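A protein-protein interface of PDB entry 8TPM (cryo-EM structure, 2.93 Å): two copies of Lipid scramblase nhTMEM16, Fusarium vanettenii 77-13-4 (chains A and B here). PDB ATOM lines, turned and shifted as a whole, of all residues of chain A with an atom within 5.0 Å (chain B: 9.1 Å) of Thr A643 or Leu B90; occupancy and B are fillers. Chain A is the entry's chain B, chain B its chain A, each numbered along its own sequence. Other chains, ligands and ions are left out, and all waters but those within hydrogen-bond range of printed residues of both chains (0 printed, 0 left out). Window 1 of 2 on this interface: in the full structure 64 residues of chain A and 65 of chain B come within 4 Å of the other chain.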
ATOM      1  N   GLU A 639     -15.174 -30.778   1.927  1.00  0.00           N
ATOM      2  CA  GLU A 639     -14.227 -31.522   1.100  1.00  0.00           C
ATOM      3  C   GLU A 639     -12.797 -31.243   1.542  1.00  0.00           C
ATOM      4  O   GLU A 639     -11.955 -32.150   1.567  1.00  0.00           O
ATOM      5  CB  GLU A 639     -14.459 -31.168  -0.376  1.00  0.00           C
ATOM      6  CG  GLU A 639     -13.953 -32.169  -1.432  1.00  0.00           C
ATOM      7  CD  GLU A 639     -12.444 -32.192  -1.655  1.00  0.00           C
ATOM      8  OE1 GLU A 639     -11.700 -31.440  -0.998  1.00  0.00           O
ATOM      9  OE2 GLU A 639     -11.997 -32.985  -2.512  1.00  0.00           O
ATOM     10  N   ARG A 640     -12.507 -29.990   1.902  1.00  0.00           N
ATOM     11  CA  ARG A 640     -11.181 -29.643   2.401  1.00  0.00           C
ATOM     12  C   ARG A 640     -10.870 -30.378   3.699  1.00  0.00           C
ATOM     13  O   ARG A 640      -9.757 -30.881   3.883  1.00  0.00           O
ATOM     14  CB  ARG A 640     -11.082 -28.130   2.600  1.00  0.00           C
ATOM     15  CG  ARG A 640      -9.698 -27.638   2.982  1.00  0.00           C
ATOM     16  CD  ARG A 640      -9.713 -26.148   3.278  1.00  0.00           C
ATOM     17  NE  ARG A 640      -9.913 -25.356   2.070  1.00  0.00           N
ATOM     18  CZ  ARG A 640     -10.504 -24.170   2.040  1.00  0.00           C
ATOM     19  NH1 ARG A 640     -10.971 -23.603   3.142  1.00  0.00           N
ATOM     20  NH2 ARG A 640     -10.631 -23.536   0.879  1.00  0.00           N
ATOM     21  N   PHE A 641     -11.842 -30.451   4.612  1.00  0.00           N
ATOM     22  CA  PHE A 641     -11.664 -31.233   5.834  1.00  0.00           C
ATOM     23  C   PHE A 641     -11.366 -32.690   5.495  1.00  0.00           C
ATOM     24  O   PHE A 641     -10.436 -33.292   6.051  1.00  0.00           O
ATOM     25  CB  PHE A 641     -12.926 -31.119   6.699  1.00  0.00           C
ATOM     26  CG  PHE A 641     -12.793 -31.665   8.115  1.00  0.00           C
ATOM     27  CD1 PHE A 641     -11.982 -32.743   8.426  1.00  0.00           C
ATOM     28  CD2 PHE A 641     -13.503 -31.076   9.142  1.00  0.00           C
ATOM     29  CE1 PHE A 641     -11.884 -33.212   9.719  1.00  0.00           C
ATOM     30  CE2 PHE A 641     -13.411 -31.549  10.439  1.00  0.00           C
ATOM     31  CZ  PHE A 641     -12.599 -32.615  10.725  1.00  0.00           C
ATOM     32  N   GLN A 642     -12.155 -33.274   4.590  1.00  0.00           N
ATOM     33  CA  GLN A 642     -11.991 -34.686   4.264  1.00  0.00           C
ATOM     34  C   GLN A 642     -10.606 -34.960   3.690  1.00  0.00           C
ATOM     35  O   GLN A 642      -9.929 -35.912   4.096  1.00  0.00           O
ATOM     36  CB  GLN A 642     -13.081 -35.129   3.287  1.00  0.00           C
ATOM     37  CG  GLN A 642     -14.488 -35.257   3.885  1.00  0.00           C
ATOM     38  CD  GLN A 642     -14.544 -36.009   5.211  1.00  0.00           C
ATOM     39  OE1 GLN A 642     -13.672 -36.818   5.530  1.00  0.00           O
ATOM     40  NE2 GLN A 642     -15.584 -35.738   5.990  1.00  0.00           N
ATOM     41  N   THR A 643     -10.159 -34.119   2.753  1.00  0.00           N
ATOM     42  CA  THR A 643      -8.844 -34.338   2.160  1.00  0.00           C
ATOM     43  C   THR A 643      -7.725 -34.049   3.155  1.00  0.00           C
ATOM     44  O   THR A 643      -6.675 -34.701   3.106  1.00  0.00           O
ATOM     45  CB  THR A 643      -8.679 -33.504   0.886  1.00  0.00           C
ATOM     46  OG1 THR A 643      -7.476 -33.892   0.211  1.00  0.00           O
ATOM     47  CG2 THR A 643      -8.620 -32.019   1.194  1.00  0.00           C
ATOM     48  N   LYS A 644      -7.936 -33.111   4.084  1.00  0.00           N
ATOM     49  CA  LYS A 644      -6.940 -32.863   5.120  1.00  0.00           C
ATOM     50  C   LYS A 644      -6.766 -34.084   6.009  1.00  0.00           C
ATOM     51  O   LYS A 644      -5.638 -34.504   6.293  1.00  0.00           O
ATOM     52  CB  LYS A 644      -7.343 -31.645   5.952  1.00  0.00           C
ATOM     53  CG  LYS A 644      -6.523 -31.457   7.217  1.00  0.00           C
ATOM     54  CD  LYS A 644      -6.439 -29.991   7.607  1.00  0.00           C
ATOM     55  CE  LYS A 644      -6.214 -29.828   9.100  1.00  0.00           C
ATOM     56  NZ  LYS A 644      -4.872 -29.256   9.401  1.00  0.00           N
ATOM     57  N   LYS A 645      -7.879 -34.676   6.452  1.00  0.00           N
ATOM     58  CA  LYS A 645      -7.787 -35.889   7.262  1.00  0.00           C
ATOM     59  C   LYS A 645      -7.172 -37.038   6.476  1.00  0.00           C
ATOM     60  O   LYS A 645      -6.379 -37.814   7.020  1.00  0.00           O
ATOM     61  CB  LYS A 645      -9.157 -36.292   7.801  1.00  0.00           C
ATOM     62  CG  LYS A 645      -9.122 -36.709   9.266  1.00  0.00           C
ATOM     63  CD  LYS A 645     -10.276 -36.135  10.058  1.00  0.00           C
ATOM     64  CE  LYS A 645     -11.580 -36.837   9.720  1.00  0.00           C
ATOM     65  NZ  LYS A 645     -12.679 -36.435  10.641  1.00  0.00           N
ATOM     66  N   ARG A 646      -7.531 -37.170   5.196  1.00  0.00           N
ATOM     67  CA  ARG A 646      -6.977 -38.252   4.389  1.00  0.00           C
ATOM     68  C   ARG A 646      -5.464 -38.117   4.259  1.00  0.00           C
ATOM     69  O   ARG A 646      -4.723 -39.092   4.437  1.00  0.00           O
ATOM     70  CB  ARG A 646      -7.644 -38.273   3.014  1.00  0.00           C
ATOM     71  CG  ARG A 646      -7.590 -39.623   2.320  1.00  0.00           C
ATOM     72  CD  ARG A 646      -6.518 -39.652   1.242  1.00  0.00           C
ATOM     73  NE  ARG A 646      -6.422 -38.384   0.530  1.00  0.00           N
ATOM     74  CZ  ARG A 646      -7.260 -37.992  -0.420  1.00  0.00           C
ATOM     75  NH1 ARG A 646      -8.275 -38.750  -0.803  1.00  0.00           N
ATOM     76  NH2 ARG A 646      -7.074 -36.809  -1.003  1.00  0.00           N
ATOM     77  N   LEU A 647      -4.983 -36.905   3.970  1.00  0.00           N
ATOM     78  CA  LEU A 647      -3.545 -36.693   3.845  1.00  0.00           C
ATOM     79  C   LEU A 647      -2.832 -36.835   5.183  1.00  0.00           C
ATOM     80  O   LEU A 647      -1.693 -37.316   5.226  1.00  0.00           O
ATOM     81  CB  LEU A 647      -3.260 -35.320   3.235  1.00  0.00           C
ATOM     82  CG  LEU A 647      -3.162 -35.221   1.709  1.00  0.00           C
ATOM     83  CD1 LEU A 647      -1.960 -36.003   1.204  1.00  0.00           C
ATOM     84  CD2 LEU A 647      -4.434 -35.689   1.021  1.00  0.00           C
ATOM     85  N   LEU A 648      -3.471 -36.426   6.282  1.00  0.00           N
ATOM     86  CA  LEU A 648      -2.834 -36.543   7.589  1.00  0.00           C
ATOM     87  C   LEU A 648      -2.720 -37.999   8.021  1.00  0.00           C
ATOM     88  O   LEU A 648      -1.697 -38.407   8.582  1.00  0.00           O
ATOM     89  CB  LEU A 648      -3.611 -35.731   8.626  1.00  0.00           C
ATOM     90  CG  LEU A 648      -3.179 -34.275   8.822  1.00  0.00           C
ATOM     91  CD1 LEU A 648      -3.588 -33.777  10.199  1.00  0.00           C
ATOM     92  CD2 LEU A 648      -1.681 -34.116   8.616  1.00  0.00           C
ATOM     93  N   TYR B  82       5.928 -30.457   6.961  1.00  0.00           N
ATOM     94  CA  TYR B  82       4.985 -31.118   6.065  1.00  0.00           C
ATOM     95  C   TYR B  82       3.555 -30.676   6.349  1.00  0.00           C
ATOM     96  O   TYR B  82       2.790 -30.395   5.418  1.00  0.00           O
ATOM     97  CB  TYR B  82       5.110 -32.636   6.194  1.00  0.00           C
ATOM     98  CG  TYR B  82       3.876 -33.385   5.742  1.00  0.00           C
ATOM     99  CD1 TYR B  82       3.582 -33.529   4.394  1.00  0.00           C
ATOM    100  CD2 TYR B  82       3.004 -33.946   6.666  1.00  0.00           C
ATOM    101  CE1 TYR B  82       2.455 -34.210   3.976  1.00  0.00           C
ATOM    102  CE2 TYR B  82       1.874 -34.628   6.257  1.00  0.00           C
ATOM    103  CZ  TYR B  82       1.605 -34.757   4.912  1.00  0.00           C
ATOM    104  OH  TYR B  82       0.482 -35.436   4.501  1.00  0.00           O
ATOM    105  N   ARG B  83       3.180 -30.603   7.627  1.00  0.00           N
ATOM    106  CA  ARG B  83       1.835 -30.157   7.979  1.00  0.00           C
ATOM    107  C   ARG B  83       1.602 -28.714   7.547  1.00  0.00           C
ATOM    108  O   ARG B  83       0.527 -28.374   7.035  1.00  0.00           O
ATOM    109  CB  ARG B  83       1.608 -30.311   9.483  1.00  0.00           C
ATOM    110  CG  ARG B  83       0.313 -29.692   9.984  1.00  0.00           C
ATOM    111  CD  ARG B  83       0.335 -29.515  11.492  1.00  0.00           C
ATOM    112  NE  ARG B  83       0.868 -30.690  12.170  1.00  0.00           N
ATOM    113  CZ  ARG B  83       0.126 -31.674  12.656  1.00  0.00           C
ATOM    114  NH1 ARG B  83      -1.194 -31.657  12.560  1.00  0.00           N
ATOM    115  NH2 ARG B  83       0.721 -32.701  13.255  1.00  0.00           N
ATOM    116  N   ALA B  84       2.600 -27.851   7.742  1.00  0.00           N
ATOM    117  CA  ALA B  84       2.458 -26.455   7.345  1.00  0.00           C
ATOM    118  C   ALA B  84       2.293 -26.324   5.836  1.00  0.00           C
ATOM    119  O   ALA B  84       1.438 -25.573   5.355  1.00  0.00           O
ATOM    120  CB  ALA B  84       3.662 -25.648   7.826  1.00  0.00           C
ATOM    121  N   ARG B  85       3.108 -27.051   5.068  1.00  0.00           N
ATOM    122  CA  ARG B  85       2.992 -26.984   3.617  1.00  0.00           C
ATOM    123  C   ARG B  85       1.675 -27.578   3.134  1.00  0.00           C
ATOM    124  O   ARG B  85       1.103 -27.089   2.153  1.00  0.00           O
ATOM    125  CB  ARG B  85       4.178 -27.686   2.960  1.00  0.00           C
ATOM    126  CG  ARG B  85       5.516 -27.021   3.235  1.00  0.00           C
ATOM    127  CD  ARG B  85       6.668 -27.841   2.682  1.00  0.00           C
ATOM    128  NE  ARG B  85       7.604 -27.017   1.928  1.00  0.00           N
ATOM    129  CZ  ARG B  85       8.925 -27.106   2.022  1.00  0.00           C
ATOM    130  NH1 ARG B  85       9.503 -27.981   2.829  1.00  0.00           N
ATOM    131  NH2 ARG B  85       9.683 -26.300   1.287  1.00  0.00           N
ATOM    132  N   LEU B  86       1.169 -28.611   3.811  1.00  0.00           N
ATOM    133  CA  LEU B  86      -0.154 -29.131   3.483  1.00  0.00           C
ATOM    134  C   LEU B  86      -1.224 -28.076   3.737  1.00  0.00           C
ATOM    135  O   LEU B  86      -2.149 -27.909   2.933  1.00  0.00           O
ATOM    136  CB  LEU B  86      -0.418 -30.406   4.292  1.00  0.00           C
ATOM    137  CG  LEU B  86      -1.602 -31.366   4.084  1.00  0.00           C
ATOM    138  CD1 LEU B  86      -1.497 -32.499   5.094  1.00  0.00           C
ATOM    139  CD2 LEU B  86      -2.977 -30.720   4.197  1.00  0.00           C
ATOM    140  N   GLY B  87      -1.110 -27.351   4.852  1.00  0.00           N
ATOM    141  CA  GLY B  87      -2.062 -26.288   5.130  1.00  0.00           C
ATOM    142  C   GLY B  87      -2.024 -25.183   4.092  1.00  0.00           C
ATOM    143  O   GLY B  87      -3.067 -24.665   3.683  1.00  0.00           O
ATOM    144  N   ASP B  88      -0.821 -24.803   3.656  1.00  0.00           N
ATOM    145  CA  ASP B  88      -0.704 -23.821   2.579  1.00  0.00           C
ATOM    146  C   ASP B  88      -1.296 -24.346   1.277  1.00  0.00           C
ATOM    147  O   ASP B  88      -1.938 -23.595   0.533  1.00  0.00           O
ATOM    148  CB  ASP B  88       0.758 -23.412   2.383  1.00  0.00           C
ATOM    149  CG  ASP B  88       1.458 -23.100   3.686  1.00  0.00           C
ATOM    150  OD1 ASP B  88       0.784 -23.101   4.737  1.00  0.00           O
ATOM    151  OD2 ASP B  88       2.682 -22.854   3.661  1.00  0.00           O
ATOM    152  N   TRP B  89      -1.087 -25.630   0.978  1.00  0.00           N
ATOM    153  CA  TRP B  89      -1.662 -26.209  -0.233  1.00  0.00           C
ATOM    154  C   TRP B  89      -3.181 -26.233  -0.179  1.00  0.00           C
ATOM    155  O   TRP B  89      -3.839 -26.080  -1.215  1.00  0.00           O
ATOM    156  CB  TRP B  89      -1.120 -27.622  -0.452  1.00  0.00           C
ATOM    157  CG  TRP B  89      -1.876 -28.388  -1.491  1.00  0.00           C
ATOM    158  CD1 TRP B  89      -1.893 -28.148  -2.834  1.00  0.00           C
ATOM    159  CD2 TRP B  89      -2.732 -29.515  -1.275  1.00  0.00           C
ATOM    160  NE1 TRP B  89      -2.703 -29.057  -3.467  1.00  0.00           N
ATOM    161  CE2 TRP B  89      -3.231 -29.907  -2.532  1.00  0.00           C
ATOM    162  CE3 TRP B  89      -3.124 -30.232  -0.140  1.00  0.00           C
ATOM    163  CZ2 TRP B  89      -4.099 -30.985  -2.685  1.00  0.00           C
ATOM    164  CZ3 TRP B  89      -3.986 -31.300  -0.295  1.00  0.00           C
ATOM    165  CH2 TRP B  89      -4.465 -31.667  -1.559  1.00  0.00           C
ATOM    166  N   LEU B  90      -3.753 -26.432   1.010  1.00  0.00           N
ATOM    167  CA  LEU B  90      -5.207 -26.465   1.137  1.00  0.00           C
ATOM    168  C   LEU B  90      -5.826 -25.128   0.752  1.00  0.00           C
ATOM    169  O   LEU B  90      -6.887 -25.086   0.119  1.00  0.00           O
ATOM    170  CB  LEU B  90      -5.596 -26.841   2.564  1.00  0.00           C
ATOM    171  CG  LEU B  90      -5.574 -28.330   2.911  1.00  0.00           C
ATOM    172  CD1 LEU B  90      -6.386 -28.585   4.163  1.00  0.00           C
ATOM    173  CD2 LEU B  90      -6.098 -29.161   1.751  1.00  0.00           C
ATOM    174  N   HIS B  91      -5.179 -24.027   1.123  1.00  0.00           N
ATOM    175  CA  HIS B  91      -5.687 -22.692   0.842  1.00  0.00           C
ATOM    176  C   HIS B  91      -5.171 -22.120  -0.471  1.00  0.00           C
ATOM    177  O   HIS B  91      -5.486 -20.970  -0.795  1.00  0.00           O
ATOM    178  CB  HIS B  91      -5.335 -21.747   1.996  1.00  0.00           C
ATOM    179  CG  HIS B  91      -5.891 -22.179   3.316  1.00  0.00           C
ATOM    180  ND1 HIS B  91      -5.152 -22.887   4.239  1.00  0.00           N
ATOM    181  CD2 HIS B  91      -7.116 -22.006   3.867  1.00  0.00           C
ATOM    182  CE1 HIS B  91      -5.897 -23.131   5.303  1.00  0.00           C
ATOM    183  NE2 HIS B  91      -7.092 -22.607   5.103  1.00  0.00           N
ATOM    184  N   GLY B  92      -4.391 -22.885  -1.230  1.00  0.00           N
ATOM    185  CA  GLY B  92      -3.928 -22.448  -2.529  1.00  0.00           C
ATOM    186  C   GLY B  92      -2.652 -21.638  -2.534  1.00  0.00           C
ATOM    187  O   GLY B  92      -2.362 -20.983  -3.542  1.00  0.00           O
ATOM    188  N   VAL B  93      -1.881 -21.653  -1.447  1.00  0.00           N
ATOM    189  CA  VAL B  93      -0.625 -20.910  -1.419  1.00  0.00           C
ATOM    190  C   VAL B  93       0.380 -21.529  -2.384  1.00  0.00           C
ATOM    191  O   VAL B  93       1.022 -20.825  -3.173  1.00  0.00           O
ATOM    192  CB  VAL B  93      -0.068 -20.846   0.014  1.00  0.00           C
ATOM    193  CG1 VAL B  93       1.343 -20.284   0.013  1.00  0.00           C
ATOM    194  CG2 VAL B  93      -0.980 -20.011   0.898  1.00  0.00           C
ATOM    195  N   ARG B  94       0.526 -22.848  -2.341  1.00  0.00           N
ATOM    196  CA  ARG B  94       1.405 -23.577  -3.242  1.00  0.00           C
ATOM    197  C   ARG B  94       0.572 -24.342  -4.267  1.00  0.00           C
ATOM    198  O   ARG B  94      -0.655 -24.229  -4.319  1.00  0.00           O
ATOM    199  CB  ARG B  94       2.329 -24.512  -2.459  1.00  0.00           C
ATOM    200  CG  ARG B  94       1.627 -25.358  -1.416  1.00  0.00           C
ATOM    201  CD  ARG B  94       2.532 -26.474  -0.925  1.00  0.00           C
ATOM    202  NE  ARG B  94       3.895 -26.008  -0.709  1.00  0.00           N
ATOM    203  CZ  ARG B  94       4.981 -26.675  -1.078  1.00  0.00           C
ATOM    204  NH1 ARG B  94       4.900 -27.846  -1.687  1.00  0.00           N
ATOM    205  NH2 ARG B  94       6.179 -26.152  -0.828  1.00  0.00           N
ATOM    206  N   VAL B  95       1.256 -25.131  -5.089  1.00  0.00           N
ATOM    207  CA  VAL B  95       0.614 -25.799  -6.217  1.00  0.00           C
ATOM    208  C   VAL B  95       0.033 -27.150  -5.818  1.00  0.00           C
ATOM    209  O   VAL B  95      -1.171 -27.382  -5.952  1.00  0.00           O
ATOM    210  CB  VAL B  95       1.611 -25.934  -7.388  1.00  0.00           C
ATOM    211  CG1 VAL B  95       1.666 -24.640  -8.181  1.00  0.00           C
ATOM    212  CG2 VAL B  95       2.996 -26.299  -6.872  1.00  0.00           C
ATOM    213  N   SER B  96       0.864 -28.064  -5.322  1.00  0.00           N
ATOM    214  CA  SER B  96       0.443 -29.431  -5.048  1.00  0.00           C
ATOM    215  C   SER B  96       0.906 -29.845  -3.656  1.00  0.00           C
ATOM    216  O   SER B  96       1.508 -29.063  -2.915  1.00  0.00           O
ATOM    217  CB  SER B  96       0.990 -30.395  -6.109  1.00  0.00           C
ATOM    218  OG  SER B  96       2.402 -30.491  -6.032  1.00  0.00           O
ATOM    219  N   ALA B  97       0.608 -31.095  -3.305  1.00  0.00           N
ATOM    220  CA  ALA B  97       1.029 -31.637  -2.025  1.00  0.00           C
ATOM    221  C   ALA B  97       2.554 -31.724  -1.971  1.00  0.00           C
ATOM    222  O   ALA B  97       3.208 -31.941  -2.996  1.00  0.00           O
ATOM    223  CB  ALA B  97       0.413 -33.018  -1.804  1.00  0.00           C
ATOM    224  N   PRO B  98       3.151 -31.546  -0.787  1.00  0.00           N
ATOM    225  CA  PRO B  98       4.618 -31.511  -0.701  1.00  0.00           C
ATOM    226  C   PRO B  98       5.273 -32.831  -1.075  1.00  0.00           C
ATOM    227  O   PRO B  98       6.038 -32.899  -2.042  1.00  0.00           O
ATOM    228  CB  PRO B  98       4.879 -31.165   0.773  1.00  0.00           C
ATOM    229  CG  PRO B  98       3.557 -30.728   1.330  1.00  0.00           C
ATOM    230  CD  PRO B  98       2.517 -31.425   0.534  1.00  0.00           C
ATOM    231  N   ARG B 250       0.915 -15.915  -1.872  1.00  0.00           N
ATOM    232  CA  ARG B 250      -0.404 -15.568  -2.383  1.00  0.00           C
ATOM    233  C   ARG B 250      -1.465 -16.418  -1.698  1.00  0.00           C
ATOM    234  O   ARG B 250      -1.339 -17.643  -1.617  1.00  0.00           O
ATOM    235  CB  ARG B 250      -0.458 -15.767  -3.896  1.00  0.00           C
ATOM    236  CG  ARG B 250      -1.350 -14.770  -4.619  1.00  0.00           C
ATOM    237  CD  ARG B 250      -2.183 -15.447  -5.695  1.00  0.00           C
ATOM    238  NE  ARG B 250      -1.374 -16.289  -6.568  1.00  0.00           N
ATOM    239  CZ  ARG B 250      -1.511 -17.604  -6.678  1.00  0.00           C
ATOM    240  NH1 ARG B 250      -2.420 -18.265  -5.982  1.00  0.00           N
ATOM    241  NH2 ARG B 250      -0.711 -18.271  -7.506  1.00  0.00           N
ATOM    242  N   GLY B 251      -2.515 -15.766  -1.205  1.00  0.00           N
ATOM    243  CA  GLY B 251      -3.569 -16.465  -0.503  1.00  0.00           C
ATOM    244  C   GLY B 251      -3.276 -16.788   0.942  1.00  0.00           C
ATOM    245  O   GLY B 251      -4.000 -17.594   1.538  1.00  0.00           O
ATOM    246  N   SER B 254      -6.048 -16.082   3.459  1.00  0.00           N
ATOM    247  CA  SER B 254      -7.114 -17.067   3.598  1.00  0.00           C
ATOM    248  C   SER B 254      -6.874 -17.987   4.789  1.00  0.00           C
ATOM    249  O   SER B 254      -7.830 -18.545   5.341  1.00  0.00           O
ATOM    250  CB  SER B 254      -7.246 -17.885   2.314  1.00  0.00           C
ATOM    251  OG  SER B 254      -7.859 -17.124   1.286  1.00  0.00           O
ATOM    252  N   ILE B 255      -5.618 -18.158   5.196  1.00  0.00           N
ATOM    253  CA  ILE B 255      -5.310 -18.987   6.354  1.00  0.00           C
ATOM    254  C   ILE B 255      -5.720 -18.252   7.623  1.00  0.00           C
ATOM    255  O   ILE B 255      -5.326 -17.101   7.848  1.00  0.00           O
ATOM    256  CB  ILE B 255      -3.817 -19.346   6.380  1.00  0.00           C
ATOM    257  CG1 ILE B 255      -3.443 -20.157   5.139  1.00  0.00           C
ATOM    258  CG2 ILE B 255      -3.474 -20.113   7.646  1.00  0.00           C
ATOM    259  CD1 ILE B 255      -1.993 -20.585   5.106  1.00  0.00           C
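The backbone carbonyl oxygen (O) of Leu A647 is in hydrogen-bond range of the side-chain hydroxyl (OH) of Tyr B82, at 3.0 Å.
OG1 of Thr A643 is in hydrogen-bond range of NH2 of Arg A646, at 3.2 Å.
Among the printed residues, pairs that only touch across the chains: Arg A640 with Leu B90, Thr A643 with Leu B90, Lys A644 with Leu B90, Leu A647 with Leu B86, Leu A648 with Arg B83 and Leu A648 with Leu B86.
Thr A643 touches one residue of chain B.
Of chain A, only Arg A640, Thr A643 and Lys A644 come within 4 Å of Leu B90.
Of the printed residues of chain A, Arg B83 touches Leu A648 (3.97 Å).
Of the printed residues of chain A, Tyr B82 touches Leu A647 (3.0 Å).
Of the printed residues of chain B, Leu A648 touches Arg B83 and Leu B86.
Gly B92 touches none of the printed residues of chain A.
The nearest printed residue of chain A that does not touch Leu B90 is Phe A641 (5.8 Å).
The nearest printed residue of chain A that does not touch Leu B86 is Lys A644 (4.6 Å).
Among the printed residues, 7 pairs touch across the chains.
Among the printed residues, no Asp or Glu carboxylate lies within 4 Å of a Lys or Arg side-chain nitrogen of the other chain.
No position is printed for both chains.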
